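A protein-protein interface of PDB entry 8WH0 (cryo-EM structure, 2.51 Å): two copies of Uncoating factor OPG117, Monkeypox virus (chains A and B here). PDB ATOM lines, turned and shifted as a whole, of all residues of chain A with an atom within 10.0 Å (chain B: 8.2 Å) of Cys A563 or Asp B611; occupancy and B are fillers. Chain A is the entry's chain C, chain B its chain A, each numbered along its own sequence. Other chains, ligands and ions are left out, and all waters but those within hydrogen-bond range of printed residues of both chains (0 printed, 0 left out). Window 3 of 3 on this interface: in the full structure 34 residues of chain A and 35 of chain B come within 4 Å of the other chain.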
ATOM      1  N   GLN A 529      -1.022   7.574  -2.369  1.00  0.00           N
ATOM      2  CA  GLN A 529      -0.182   6.527  -1.803  1.00  0.00           C
ATOM      3  C   GLN A 529      -0.468   5.152  -2.390  1.00  0.00           C
ATOM      4  O   GLN A 529       0.270   4.208  -2.090  1.00  0.00           O
ATOM      5  CB  GLN A 529      -0.348   6.485  -0.283  1.00  0.00           C
ATOM      6  CG  GLN A 529      -1.714   6.928   0.204  1.00  0.00           C
ATOM      7  CD  GLN A 529      -1.768   7.100   1.708  1.00  0.00           C
ATOM      8  OE1 GLN A 529      -1.006   7.877   2.283  1.00  0.00           O
ATOM      9  NE2 GLN A 529      -2.672   6.373   2.354  1.00  0.00           N
ATOM     10  N   LEU A 558       2.650   9.828   4.342  1.00  0.00           N
ATOM     11  CA  LEU A 558       2.707   8.386   4.530  1.00  0.00           C
ATOM     12  C   LEU A 558       1.899   7.996   5.764  1.00  0.00           C
ATOM     13  O   LEU A 558       2.101   8.577   6.840  1.00  0.00           O
ATOM     14  CB  LEU A 558       4.152   7.917   4.689  1.00  0.00           C
ATOM     15  CG  LEU A 558       4.882   7.354   3.470  1.00  0.00           C
ATOM     16  CD1 LEU A 558       6.167   6.670   3.905  1.00  0.00           C
ATOM     17  CD2 LEU A 558       3.994   6.393   2.703  1.00  0.00           C
ATOM     18  N   PRO A 559       0.990   7.029   5.661  1.00  0.00           N
ATOM     19  CA  PRO A 559       0.286   6.548   6.856  1.00  0.00           C
ATOM     20  C   PRO A 559       1.217   5.740   7.742  1.00  0.00           C
ATOM     21  O   PRO A 559       1.234   4.507   7.679  1.00  0.00           O
ATOM     22  CB  PRO A 559      -0.844   5.682   6.284  1.00  0.00           C
ATOM     23  CG  PRO A 559      -0.928   6.048   4.833  1.00  0.00           C
ATOM     24  CD  PRO A 559       0.460   6.420   4.432  1.00  0.00           C
ATOM     25  N   ASP A 560       1.998   6.432   8.566  1.00  0.00           N
ATOM     26  CA  ASP A 560       3.091   5.801   9.285  1.00  0.00           C
ATOM     27  C   ASP A 560       2.590   4.631  10.130  1.00  0.00           C
ATOM     28  O   ASP A 560       1.391   4.429  10.333  1.00  0.00           O
ATOM     29  CB  ASP A 560       3.803   6.814  10.173  1.00  0.00           C
ATOM     30  N   PHE A 561       3.550   3.853  10.632  1.00  0.00           N
ATOM     31  CA  PHE A 561       3.270   2.572  11.264  1.00  0.00           C
ATOM     32  C   PHE A 561       3.659   2.554  12.736  1.00  0.00           C
ATOM     33  O   PHE A 561       3.896   1.481  13.298  1.00  0.00           O
ATOM     34  CB  PHE A 561       3.980   1.459  10.496  1.00  0.00           C
ATOM     35  CG  PHE A 561       3.652   1.449   9.035  1.00  0.00           C
ATOM     36  CD1 PHE A 561       4.410   2.184   8.138  1.00  0.00           C
ATOM     37  CD2 PHE A 561       2.573   0.731   8.560  1.00  0.00           C
ATOM     38  CE1 PHE A 561       4.105   2.191   6.795  1.00  0.00           C
ATOM     39  CE2 PHE A 561       2.264   0.732   7.216  1.00  0.00           C
ATOM     40  CZ  PHE A 561       3.031   1.463   6.332  1.00  0.00           C
ATOM     41  N   ALA A 562       3.729   3.724  13.376  1.00  0.00           N
ATOM     42  CA  ALA A 562       3.912   3.758  14.822  1.00  0.00           C
ATOM     43  C   ALA A 562       2.794   2.993  15.516  1.00  0.00           C
ATOM     44  O   ALA A 562       3.041   2.185  16.418  1.00  0.00           O
ATOM     45  CB  ALA A 562       3.969   5.206  15.311  1.00  0.00           C
ATOM     46  N   CYS A 563       1.552   3.236  15.101  1.00  0.00           N
ATOM     47  CA  CYS A 563       0.419   2.406  15.492  1.00  0.00           C
ATOM     48  C   CYS A 563       0.256   1.315  14.439  1.00  0.00           C
ATOM     49  O   CYS A 563      -0.181   1.584  13.317  1.00  0.00           O
ATOM     50  CB  CYS A 563      -0.849   3.244  15.635  1.00  0.00           C
ATOM     51  SG  CYS A 563      -1.361   4.122  14.137  1.00  0.00           S
ATOM     52  N   SER A 564       0.618   0.085  14.797  1.00  0.00           N
ATOM     53  CA  SER A 564       0.573  -1.008  13.837  1.00  0.00           C
ATOM     54  C   SER A 564      -0.863  -1.287  13.408  1.00  0.00           C
ATOM     55  O   SER A 564      -1.812  -1.108  14.175  1.00  0.00           O
ATOM     56  CB  SER A 564       1.197  -2.269  14.437  1.00  0.00           C
ATOM     57  N   GLY A 565      -1.014  -1.729  12.161  1.00  0.00           N
ATOM     58  CA  GLY A 565      -2.325  -2.043  11.626  1.00  0.00           C
ATOM     59  C   GLY A 565      -2.583  -1.463  10.251  1.00  0.00           C
ATOM     60  O   GLY A 565      -3.720  -1.485   9.768  1.00  0.00           O
ATOM     61  N   SER A 566      -1.541  -0.944   9.606  1.00  0.00           N
ATOM     62  CA  SER A 566      -1.657  -0.326   8.295  1.00  0.00           C
ATOM     63  C   SER A 566      -0.837  -1.103   7.274  1.00  0.00           C
ATOM     64  O   SER A 566       0.196  -1.695   7.602  1.00  0.00           O
ATOM     65  CB  SER A 566      -1.196   1.136   8.328  1.00  0.00           C
ATOM     66  N   LYS A 567      -1.310  -1.096   6.029  1.00  0.00           N
ATOM     67  CA  LYS A 567      -0.608  -1.792   4.959  1.00  0.00           C
ATOM     68  C   LYS A 567       0.783  -1.202   4.761  1.00  0.00           C
ATOM     69  O   LYS A 567       0.977   0.016   4.787  1.00  0.00           O
ATOM     70  CB  LYS A 567      -1.399  -1.705   3.653  1.00  0.00           C
ATOM     71  CG  LYS A 567      -2.906  -1.769   3.823  1.00  0.00           C
ATOM     72  CD  LYS A 567      -3.612  -0.990   2.726  1.00  0.00           C
ATOM     73  CE  LYS A 567      -3.941  -1.878   1.536  1.00  0.00           C
ATOM     74  NZ  LYS A 567      -5.310  -2.457   1.631  1.00  0.00           N
ATOM     75  N   LYS A 568       1.754  -2.082   4.543  1.00  0.00           N
ATOM     76  CA  LYS A 568       3.137  -1.677   4.359  1.00  0.00           C
ATOM     77  C   LYS A 568       3.405  -1.327   2.897  1.00  0.00           C
ATOM     78  O   LYS A 568       2.578  -1.558   2.011  1.00  0.00           O
ATOM     79  CB  LYS A 568       4.084  -2.784   4.823  1.00  0.00           C
ATOM     80  CG  LYS A 568       3.778  -3.322   6.211  1.00  0.00           C
ATOM     81  CD  LYS A 568       4.412  -2.463   7.290  1.00  0.00           C
ATOM     82  CE  LYS A 568       5.620  -3.153   7.903  1.00  0.00           C
ATOM     83  NZ  LYS A 568       5.323  -4.556   8.299  1.00  0.00           N
ATOM     84  N   TYR A 606       7.469  10.254   9.349  1.00  0.00           N
ATOM     85  CA  TYR A 606       7.891   8.976   9.902  1.00  0.00           C
ATOM     86  C   TYR A 606       8.672   8.201   8.851  1.00  0.00           C
ATOM     87  O   TYR A 606       8.322   8.220   7.668  1.00  0.00           O
ATOM     88  CB  TYR A 606       6.685   8.154  10.363  1.00  0.00           C
ATOM     89  CG  TYR A 606       5.853   8.826  11.430  1.00  0.00           C
ATOM     90  CD1 TYR A 606       6.176   8.701  12.772  1.00  0.00           C
ATOM     91  CD2 TYR A 606       4.746   9.594  11.091  1.00  0.00           C
ATOM     92  CE1 TYR A 606       5.417   9.313  13.746  1.00  0.00           C
ATOM     93  CE2 TYR A 606       3.983  10.208  12.057  1.00  0.00           C
ATOM     94  CZ  TYR A 606       4.323  10.066  13.382  1.00  0.00           C
ATOM     95  OH  TYR A 606       3.565  10.679  14.350  1.00  0.00           O
ATOM     96  N   VAL A 609       8.648   1.816   6.365  1.00  0.00           N
ATOM     97  CA  VAL A 609       8.837   0.417   6.723  1.00  0.00           C
ATOM     98  C   VAL A 609       8.280  -0.439   5.594  1.00  0.00           C
ATOM     99  O   VAL A 609       7.176  -0.181   5.100  1.00  0.00           O
ATOM    100  CB  VAL A 609       8.162   0.064   8.062  1.00  0.00           C
ATOM    101  CG1 VAL A 609       8.410   1.161   9.084  1.00  0.00           C
ATOM    102  CG2 VAL A 609       6.675  -0.161   7.870  1.00  0.00           C
ATOM    103  N   LEU B 532     -12.964  10.960   6.426  1.00  0.00           N
ATOM    104  CA  LEU B 532     -12.179  11.006   7.649  1.00  0.00           C
ATOM    105  C   LEU B 532     -11.681   9.644   8.105  1.00  0.00           C
ATOM    106  O   LEU B 532     -10.768   9.587   8.933  1.00  0.00           O
ATOM    107  CB  LEU B 532     -12.998  11.626   8.791  1.00  0.00           C
ATOM    108  CG  LEU B 532     -13.345  13.113   8.715  1.00  0.00           C
ATOM    109  CD1 LEU B 532     -13.944  13.575  10.030  1.00  0.00           C
ATOM    110  CD2 LEU B 532     -12.122  13.939   8.365  1.00  0.00           C
ATOM    111  N   THR B 533     -12.253   8.553   7.592  1.00  0.00           N
ATOM    112  CA  THR B 533     -11.922   7.213   8.049  1.00  0.00           C
ATOM    113  C   THR B 533     -11.480   6.267   6.944  1.00  0.00           C
ATOM    114  O   THR B 533     -10.893   5.225   7.253  1.00  0.00           O
ATOM    115  CB  THR B 533     -13.122   6.582   8.774  1.00  0.00           C
ATOM    116  OG1 THR B 533     -14.235   6.499   7.877  1.00  0.00           O
ATOM    117  CG2 THR B 533     -13.517   7.416   9.978  1.00  0.00           C
ATOM    118  N   LYS B 567     -14.188   2.665  13.703  1.00  0.00           N
ATOM    119  CA  LYS B 567     -13.003   3.105  12.980  1.00  0.00           C
ATOM    120  C   LYS B 567     -12.569   4.478  13.473  1.00  0.00           C
ATOM    121  O   LYS B 567     -13.390   5.391  13.600  1.00  0.00           O
ATOM    122  CB  LYS B 567     -13.281   3.148  11.478  1.00  0.00           C
ATOM    123  CG  LYS B 567     -13.855   1.867  10.908  1.00  0.00           C
ATOM    124  CD  LYS B 567     -13.155   1.490   9.615  1.00  0.00           C
ATOM    125  CE  LYS B 567     -13.685   2.301   8.442  1.00  0.00           C
ATOM    126  NZ  LYS B 567     -13.449   1.616   7.141  1.00  0.00           N
ATOM    127  N   LYS B 568     -11.276   4.627  13.745  1.00  0.00           N
ATOM    128  CA  LYS B 568     -10.746   5.896  14.211  1.00  0.00           C
ATOM    129  C   LYS B 568     -10.557   6.859  13.041  1.00  0.00           C
ATOM    130  O   LYS B 568     -10.632   6.484  11.868  1.00  0.00           O
ATOM    131  CB  LYS B 568      -9.424   5.686  14.943  1.00  0.00           C
ATOM    132  CG  LYS B 568      -9.490   4.655  16.051  1.00  0.00           C
ATOM    133  CD  LYS B 568      -9.583   5.319  17.409  1.00  0.00           C
ATOM    134  CE  LYS B 568      -9.136   4.380  18.516  1.00  0.00           C
ATOM    135  NZ  LYS B 568      -7.833   4.795  19.103  1.00  0.00           N
ATOM    136  N   ILE B 569     -10.314   8.122  13.376  1.00  0.00           N
ATOM    137  CA  ILE B 569     -10.001   9.130  12.369  1.00  0.00           C
ATOM    138  C   ILE B 569      -8.540   8.986  11.967  1.00  0.00           C
ATOM    139  O   ILE B 569      -7.655   8.881  12.825  1.00  0.00           O
ATOM    140  CB  ILE B 569     -10.298  10.543  12.894  1.00  0.00           C
ATOM    141  CG1 ILE B 569     -11.745  10.646  13.374  1.00  0.00           C
ATOM    142  CG2 ILE B 569     -10.018  11.576  11.817  1.00  0.00           C
ATOM    143  CD1 ILE B 569     -11.965  11.712  14.420  1.00  0.00           C
ATOM    144  N   ARG B 570      -8.285   8.977  10.664  1.00  0.00           N
ATOM    145  CA  ARG B 570      -6.928   8.848  10.151  1.00  0.00           C
ATOM    146  C   ARG B 570      -6.249  10.212  10.143  1.00  0.00           C
ATOM    147  O   ARG B 570      -6.696  11.130   9.448  1.00  0.00           O
ATOM    148  CB  ARG B 570      -6.949   8.245   8.750  1.00  0.00           C
ATOM    149  CG  ARG B 570      -7.893   7.069   8.602  1.00  0.00           C
ATOM    150  CD  ARG B 570      -7.896   6.542   7.182  1.00  0.00           C
ATOM    151  NE  ARG B 570      -6.568   6.597   6.584  1.00  0.00           N
ATOM    152  CZ  ARG B 570      -6.020   5.612   5.886  1.00  0.00           C
ATOM    153  NH1 ARG B 570      -6.658   4.472   5.680  1.00  0.00           N
ATOM    154  NH2 ARG B 570      -4.801   5.774   5.381  1.00  0.00           N
ATOM    155  N   SER B 571      -5.167  10.344  10.915  1.00  0.00           N
ATOM    156  CA  SER B 571      -4.445  11.611  10.970  1.00  0.00           C
ATOM    157  C   SER B 571      -3.878  11.995   9.609  1.00  0.00           C
ATOM    158  O   SER B 571      -3.817  13.185   9.271  1.00  0.00           O
ATOM    159  CB  SER B 571      -3.329  11.530  12.010  1.00  0.00           C
ATOM    160  OG  SER B 571      -3.775  10.878  13.183  1.00  0.00           O
ATOM    161  N   ASP B 572      -3.454  11.010   8.817  1.00  0.00           N
ATOM    162  CA  ASP B 572      -2.978  11.317   7.474  1.00  0.00           C
ATOM    163  C   ASP B 572      -4.098  11.872   6.606  1.00  0.00           C
ATOM    164  O   ASP B 572      -3.844  12.696   5.724  1.00  0.00           O
ATOM    165  CB  ASP B 572      -2.359  10.075   6.833  1.00  0.00           C
ATOM    166  CG  ASP B 572      -3.277   8.873   6.885  1.00  0.00           C
ATOM    167  OD1 ASP B 572      -3.436   8.294   7.979  1.00  0.00           O
ATOM    168  OD2 ASP B 572      -3.835   8.504   5.831  1.00  0.00           O
ATOM    169  N   ASN B 573      -5.341  11.450   6.849  1.00  0.00           N
ATOM    170  CA  ASN B 573      -6.471  12.063   6.158  1.00  0.00           C
ATOM    171  C   ASN B 573      -6.605  13.533   6.529  1.00  0.00           C
ATOM    172  O   ASN B 573      -6.883  14.373   5.668  1.00  0.00           O
ATOM    173  CB  ASN B 573      -7.760  11.307   6.475  1.00  0.00           C
ATOM    174  CG  ASN B 573      -7.971  10.118   5.563  1.00  0.00           C
ATOM    175  OD1 ASN B 573      -7.025   9.410   5.226  1.00  0.00           O
ATOM    176  ND2 ASN B 573      -9.212   9.895   5.155  1.00  0.00           N
ATOM    177  N   ILE B 574      -6.407  13.865   7.805  1.00  0.00           N
ATOM    178  CA  ILE B 574      -6.420  15.265   8.225  1.00  0.00           C
ATOM    179  C   ILE B 574      -5.340  16.045   7.487  1.00  0.00           C
ATOM    180  O   ILE B 574      -5.586  17.130   6.939  1.00  0.00           O
ATOM    181  CB  ILE B 574      -6.239  15.366   9.751  1.00  0.00           C
ATOM    182  CG1 ILE B 574      -7.329  14.578  10.480  1.00  0.00           C
ATOM    183  CG2 ILE B 574      -6.222  16.820  10.197  1.00  0.00           C
ATOM    184  CD1 ILE B 574      -8.714  15.152  10.313  1.00  0.00           C
ATOM    185  N   PRO B 608     -13.249  13.836  19.306  1.00  0.00           N
ATOM    186  CA  PRO B 608     -12.634  12.957  18.307  1.00  0.00           C
ATOM    187  C   PRO B 608     -11.554  12.072  18.909  1.00  0.00           C
ATOM    188  O   PRO B 608     -10.916  12.413  19.907  1.00  0.00           O
ATOM    189  CB  PRO B 608     -12.039  13.935  17.283  1.00  0.00           C
ATOM    190  CG  PRO B 608     -12.470  15.312  17.720  1.00  0.00           C
ATOM    191  CD  PRO B 608     -12.806  15.229  19.164  1.00  0.00           C
ATOM    192  N   VAL B 609     -11.355  10.917  18.279  1.00  0.00           N
ATOM    193  CA  VAL B 609     -10.314   9.970  18.658  1.00  0.00           C
ATOM    194  C   VAL B 609      -9.557   9.585  17.395  1.00  0.00           C
ATOM    195  O   VAL B 609     -10.170   9.154  16.410  1.00  0.00           O
ATOM    196  CB  VAL B 609     -10.889   8.723  19.352  1.00  0.00           C
ATOM    197  CG1 VAL B 609      -9.819   7.660  19.502  1.00  0.00           C
ATOM    198  CG2 VAL B 609     -11.470   9.091  20.705  1.00  0.00           C
ATOM    199  N   PHE B 610      -8.237   9.740  17.420  1.00  0.00           N
ATOM    200  CA  PHE B 610      -7.391   9.502  16.261  1.00  0.00           C
ATOM    201  C   PHE B 610      -6.518   8.272  16.484  1.00  0.00           C
ATOM    202  O   PHE B 610      -6.153   7.945  17.616  1.00  0.00           O
ATOM    203  CB  PHE B 610      -6.506  10.717  15.966  1.00  0.00           C
ATOM    204  CG  PHE B 610      -7.222  12.033  16.081  1.00  0.00           C
ATOM    205  CD1 PHE B 610      -7.269  12.708  17.289  1.00  0.00           C
ATOM    206  CD2 PHE B 610      -7.845  12.597  14.983  1.00  0.00           C
ATOM    207  CE1 PHE B 610      -7.924  13.916  17.397  1.00  0.00           C
ATOM    208  CE2 PHE B 610      -8.501  13.804  15.089  1.00  0.00           C
ATOM    209  CZ  PHE B 610      -8.539  14.464  16.297  1.00  0.00           C
ATOM    210  N   ASP B 611      -6.184   7.594  15.383  1.00  0.00           N
ATOM    211  CA  ASP B 611      -5.371   6.387  15.480  1.00  0.00           C
ATOM    212  C   ASP B 611      -3.976   6.694  16.014  1.00  0.00           C
ATOM    213  O   ASP B 611      -3.455   5.957  16.859  1.00  0.00           O
ATOM    214  CB  ASP B 611      -5.293   5.693  14.120  1.00  0.00           C
ATOM    215  CG  ASP B 611      -4.818   6.615  13.016  1.00  0.00           C
ATOM    216  OD1 ASP B 611      -4.146   7.620  13.323  1.00  0.00           O
ATOM    217  OD2 ASP B 611      -5.116   6.332  11.839  1.00  0.00           O
ATOM    218  N   ARG B 612      -3.356   7.773  15.540  1.00  0.00           N
ATOM    219  CA  ARG B 612      -2.026   8.168  15.984  1.00  0.00           C
ATOM    220  C   ARG B 612      -2.013   9.655  16.305  1.00  0.00           C
ATOM    221  O   ARG B 612      -2.670  10.450  15.629  1.00  0.00           O
ATOM    222  CB  ARG B 612      -0.967   7.852  14.923  1.00  0.00           C
ATOM    223  CG  ARG B 612       0.461   7.882  15.446  1.00  0.00           C
ATOM    224  CD  ARG B 612       1.454   8.115  14.323  1.00  0.00           C
ATOM    225  NE  ARG B 612       0.824   8.721  13.158  1.00  0.00           N
ATOM    226  CZ  ARG B 612       0.747   8.147  11.965  1.00  0.00           C
ATOM    227  NH1 ARG B 612       1.243   6.941  11.746  1.00  0.00           N
ATOM    228  NH2 ARG B 612       0.153   8.798  10.969  1.00  0.00           N
ATOM    229  N   ILE B 613      -1.255  10.027  17.335  1.00  0.00           N
ATOM    230  CA  ILE B 613      -1.164  11.404  17.802  1.00  0.00           C
ATOM    231  C   ILE B 613       0.275  11.876  17.655  1.00  0.00           C
ATOM    232  O   ILE B 613       1.205  11.197  18.105  1.00  0.00           O
ATOM    233  CB  ILE B 613      -1.632  11.544  19.263  1.00  0.00           C
ATOM    234  CG1 ILE B 613      -3.157  11.506  19.345  1.00  0.00           C
ATOM    235  CG2 ILE B 613      -1.101  12.832  19.869  1.00  0.00           C
ATOM    236  CD1 ILE B 613      -3.685  11.450  20.758  1.00  0.00           C
ATOM    237  N   ASP B 614       0.454  13.038  17.032  1.00  0.00           N
ATOM    238  CA  ASP B 614       1.769  13.647  16.890  1.00  0.00           C
ATOM    239  C   ASP B 614       1.596  15.155  16.772  1.00  0.00           C
ATOM    240  O   ASP B 614       0.480  15.666  16.660  1.00  0.00           O
ATOM    241  CB  ASP B 614       2.527  13.080  15.686  1.00  0.00           C
ATOM    242  CG  ASP B 614       1.737  13.177  14.396  1.00  0.00           C
ATOM    243  OD1 ASP B 614       0.572  12.726  14.371  1.00  0.00           O
ATOM    244  OD2 ASP B 614       2.281  13.699  13.403  1.00  0.00           O
ATOM    245  N   LEU B 617      -0.482  16.589  13.810  1.00  0.00           N
ATOM    246  CA  LEU B 617      -1.934  16.576  13.943  1.00  0.00           C
ATOM    247  C   LEU B 617      -2.415  17.609  14.953  1.00  0.00           C
ATOM    248  O   LEU B 617      -3.447  18.253  14.739  1.00  0.00           O
ATOM    249  CB  LEU B 617      -2.410  15.179  14.340  1.00  0.00           C
ATOM    250  CG  LEU B 617      -3.867  15.045  14.785  1.00  0.00           C
ATOM    251  CD1 LEU B 617      -4.754  14.678  13.610  1.00  0.00           C
ATOM    252  CD2 LEU B 617      -3.986  14.016  15.892  1.00  0.00           C
ATOM    253  N   ASP B 695      -7.692  13.732  24.137  1.00  0.00           N
ATOM    254  CA  ASP B 695      -6.658  12.852  23.600  1.00  0.00           C
ATOM    255  C   ASP B 695      -5.279  13.493  23.704  1.00  0.00           C
ATOM    256  O   ASP B 695      -4.320  12.865  24.165  1.00  0.00           O
ATOM    257  CB  ASP B 695      -6.975  12.505  22.145  1.00  0.00           C
ATOM    258  CG  ASP B 695      -7.390  11.061  21.964  1.00  0.00           C
ATOM    259  OD1 ASP B 695      -7.575  10.361  22.981  1.00  0.00           O
ATOM    260  OD2 ASP B 695      -7.525  10.624  20.801  1.00  0.00           O
ATOM    261  N   TYR B 699       0.144  14.398  25.953  1.00  0.00           N
ATOM    262  CA  TYR B 699       1.306  14.930  25.252  1.00  0.00           C
ATOM    263  C   TYR B 699       1.611  16.348  25.706  1.00  0.00           C
ATOM    264  O   TYR B 699       2.758  16.677  26.032  1.00  0.00           O
ATOM    265  CB  TYR B 699       1.082  14.871  23.741  1.00  0.00           C
ATOM    266  CG  TYR B 699       1.006  13.461  23.204  1.00  0.00           C
ATOM    267  CD1 TYR B 699      -0.114  12.671  23.427  1.00  0.00           C
ATOM    268  CD2 TYR B 699       2.063  12.911  22.493  1.00  0.00           C
ATOM    269  CE1 TYR B 699      -0.185  11.379  22.945  1.00  0.00           C
ATOM    270  CE2 TYR B 699       2.001  11.619  22.007  1.00  0.00           C
ATOM    271  CZ  TYR B 699       0.876  10.859  22.236  1.00  0.00           C
ATOM    272  OH  TYR B 699       0.810   9.572  21.753  1.00  0.00           O
ATOM    273  N   HIS B 754      -1.260   3.243  28.310  1.00  0.00           N
ATOM    274  CA  HIS B 754      -0.929   3.126  26.894  1.00  0.00           C
ATOM    275  C   HIS B 754      -0.096   4.309  26.420  1.00  0.00           C
ATOM    276  O   HIS B 754       0.878   4.131  25.681  1.00  0.00           O
ATOM    277  CB  HIS B 754      -2.205   3.001  26.061  1.00  0.00           C
ATOM    278  CG  HIS B 754      -1.956   2.871  24.590  1.00  0.00           C
ATOM    279  ND1 HIS B 754      -1.672   3.953  23.785  1.00  0.00           N
ATOM    280  CD2 HIS B 754      -1.945   1.787  23.780  1.00  0.00           C
ATOM    281  CE1 HIS B 754      -1.497   3.541  22.542  1.00  0.00           C
ATOM    282  NE2 HIS B 754      -1.657   2.230  22.512  1.00  0.00           N
ATOM    283  N   SER B 758       3.687   4.057  25.034  1.00  0.00           N
ATOM    284  CA  SER B 758       3.978   4.509  23.681  1.00  0.00           C
ATOM    285  C   SER B 758       5.099   5.537  23.674  1.00  0.00           C
ATOM    286  O   SER B 758       5.986   5.492  22.816  1.00  0.00           O
ATOM    287  CB  SER B 758       2.716   5.084  23.038  1.00  0.00           C
ATOM    288  OG  SER B 758       1.780   4.059  22.752  1.00  0.00           O
ATOM    289  N   ARG B 762       8.628   4.961  21.819  1.00  0.00           N
ATOM    290  CA  ARG B 762       8.991   5.871  20.740  1.00  0.00           C
ATOM    291  C   ARG B 762      10.333   6.541  20.998  1.00  0.00           C
ATOM    292  O   ARG B 762      11.159   6.658  20.085  1.00  0.00           O
ATOM    293  CB  ARG B 762       7.896   6.922  20.559  1.00  0.00           C
ATOM    294  CG  ARG B 762       7.667   7.355  19.122  1.00  0.00           C
ATOM    295  CD  ARG B 762       6.858   8.640  19.064  1.00  0.00           C
ATOM    296  NE  ARG B 762       5.608   8.475  18.331  1.00  0.00           N
ATOM    297  CZ  ARG B 762       4.732   9.447  18.115  1.00  0.00           C
ATOM    298  NH1 ARG B 762       4.936  10.674  18.564  1.00  0.00           N
ATOM    299  NH2 ARG B 762       3.623   9.180  17.432  1.00  0.00           N
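The backbone carbonyl oxygen (O) of Ile B569 is in hydrogen-bond range of the backbone NH (N) of Asp B611, 3.2 Å away. The guanidinium group (NH2) of Arg B570 lies within salt-bridge range of the side-chain carboxylate (OD2) of Asp B572 (2.9 Å). NE of Arg B570 lies within hydrogen-bond range of OD1 of Asn B573, 3.2 Å away. The side-chain hydroxyl of Ser B571 is in hydrogen-bond range of the side-chain carboxylate of Asp B611, at 3.3 Å. O of Arg B612 lies within hydrogen-bond range of OG of Ser B571, at 2.7 Å. O of Ile B613 is in hydrogen-bond range of NH2 of Arg B762 (3.2 Å).
Of the 23 printed residues of chain B, 6 touch a printed residue of chain A. Of the 14 printed residues of chain A, 6 touch a printed residue of chain B. Printed residues of chain A that touch a printed residue of chain B: Gln A529, Pro A559, Asp A560, Ala A562, Cys A563 and Tyr A606. Hydrophobic or aromatic side chains of chain A that line the printed part of chain B: Pro A559, Ala A562 and Tyr A606. Among the printed residues, no Asp or Glu carboxylate lies within 4 Å of a Lys or Arg side-chain nitrogen of the other chain.
3 positions are printed for both chains. Of the 10 pairs that touch across the chains among the printed residues, none has its exchanged pair printed and touching as well.
Of chain B, only Asp B611 and Arg B612 come within 4 Å of Cys A563. Asp B611 touches just one residue of chain A: Cys A563. Of chain B, only Arg B612 comes within 4 Å of Ala A562. No residue of chain B comes within 4 Å of Ser A564. Printed residues of chain A within 4 Å of Asp B614: Tyr A606 (2.9 Å). Of the printed residues of chain B, Pro A559 touches Arg B570 (3.9 Å) and Asp B572 (3.9 Å). The nearest printed residue of chain B that does not touch Cys A563 is Arg B762 (6.7 Å). The nearest printed residue of chain B that does not touch Asp A560 is Asp B572 (5.8 Å).
The guanidinium group (NH1) of Arg B612 is in hydrogen-bond range of the backbone carbonyl oxygen (O) of Asp A560 (2.9 Å). The side-chain carboxylate of Asp B614 lies close to the side-chain hydroxyl of Tyr A606. The guanidinium group (NH2) of Arg B762 lies within hydrogen-bond range of the side-chain hydroxyl (OH) of Tyr A606 (3.4 Å).
Among the printed residues, merely in contact across the chains: Gln A529 with Arg B570 (3.7 Å), Pro A559 with Arg B570 (3.9 Å), Pro A559 with Asp B572 (3.9 Å), Ala A562 with Arg B612 (3.97 Å), Cys A563 with Asp B611 (3.9 Å), Cys A563 with Arg B612 (3.8 Å) and Tyr A606 with Arg B612 (3.3 Å).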
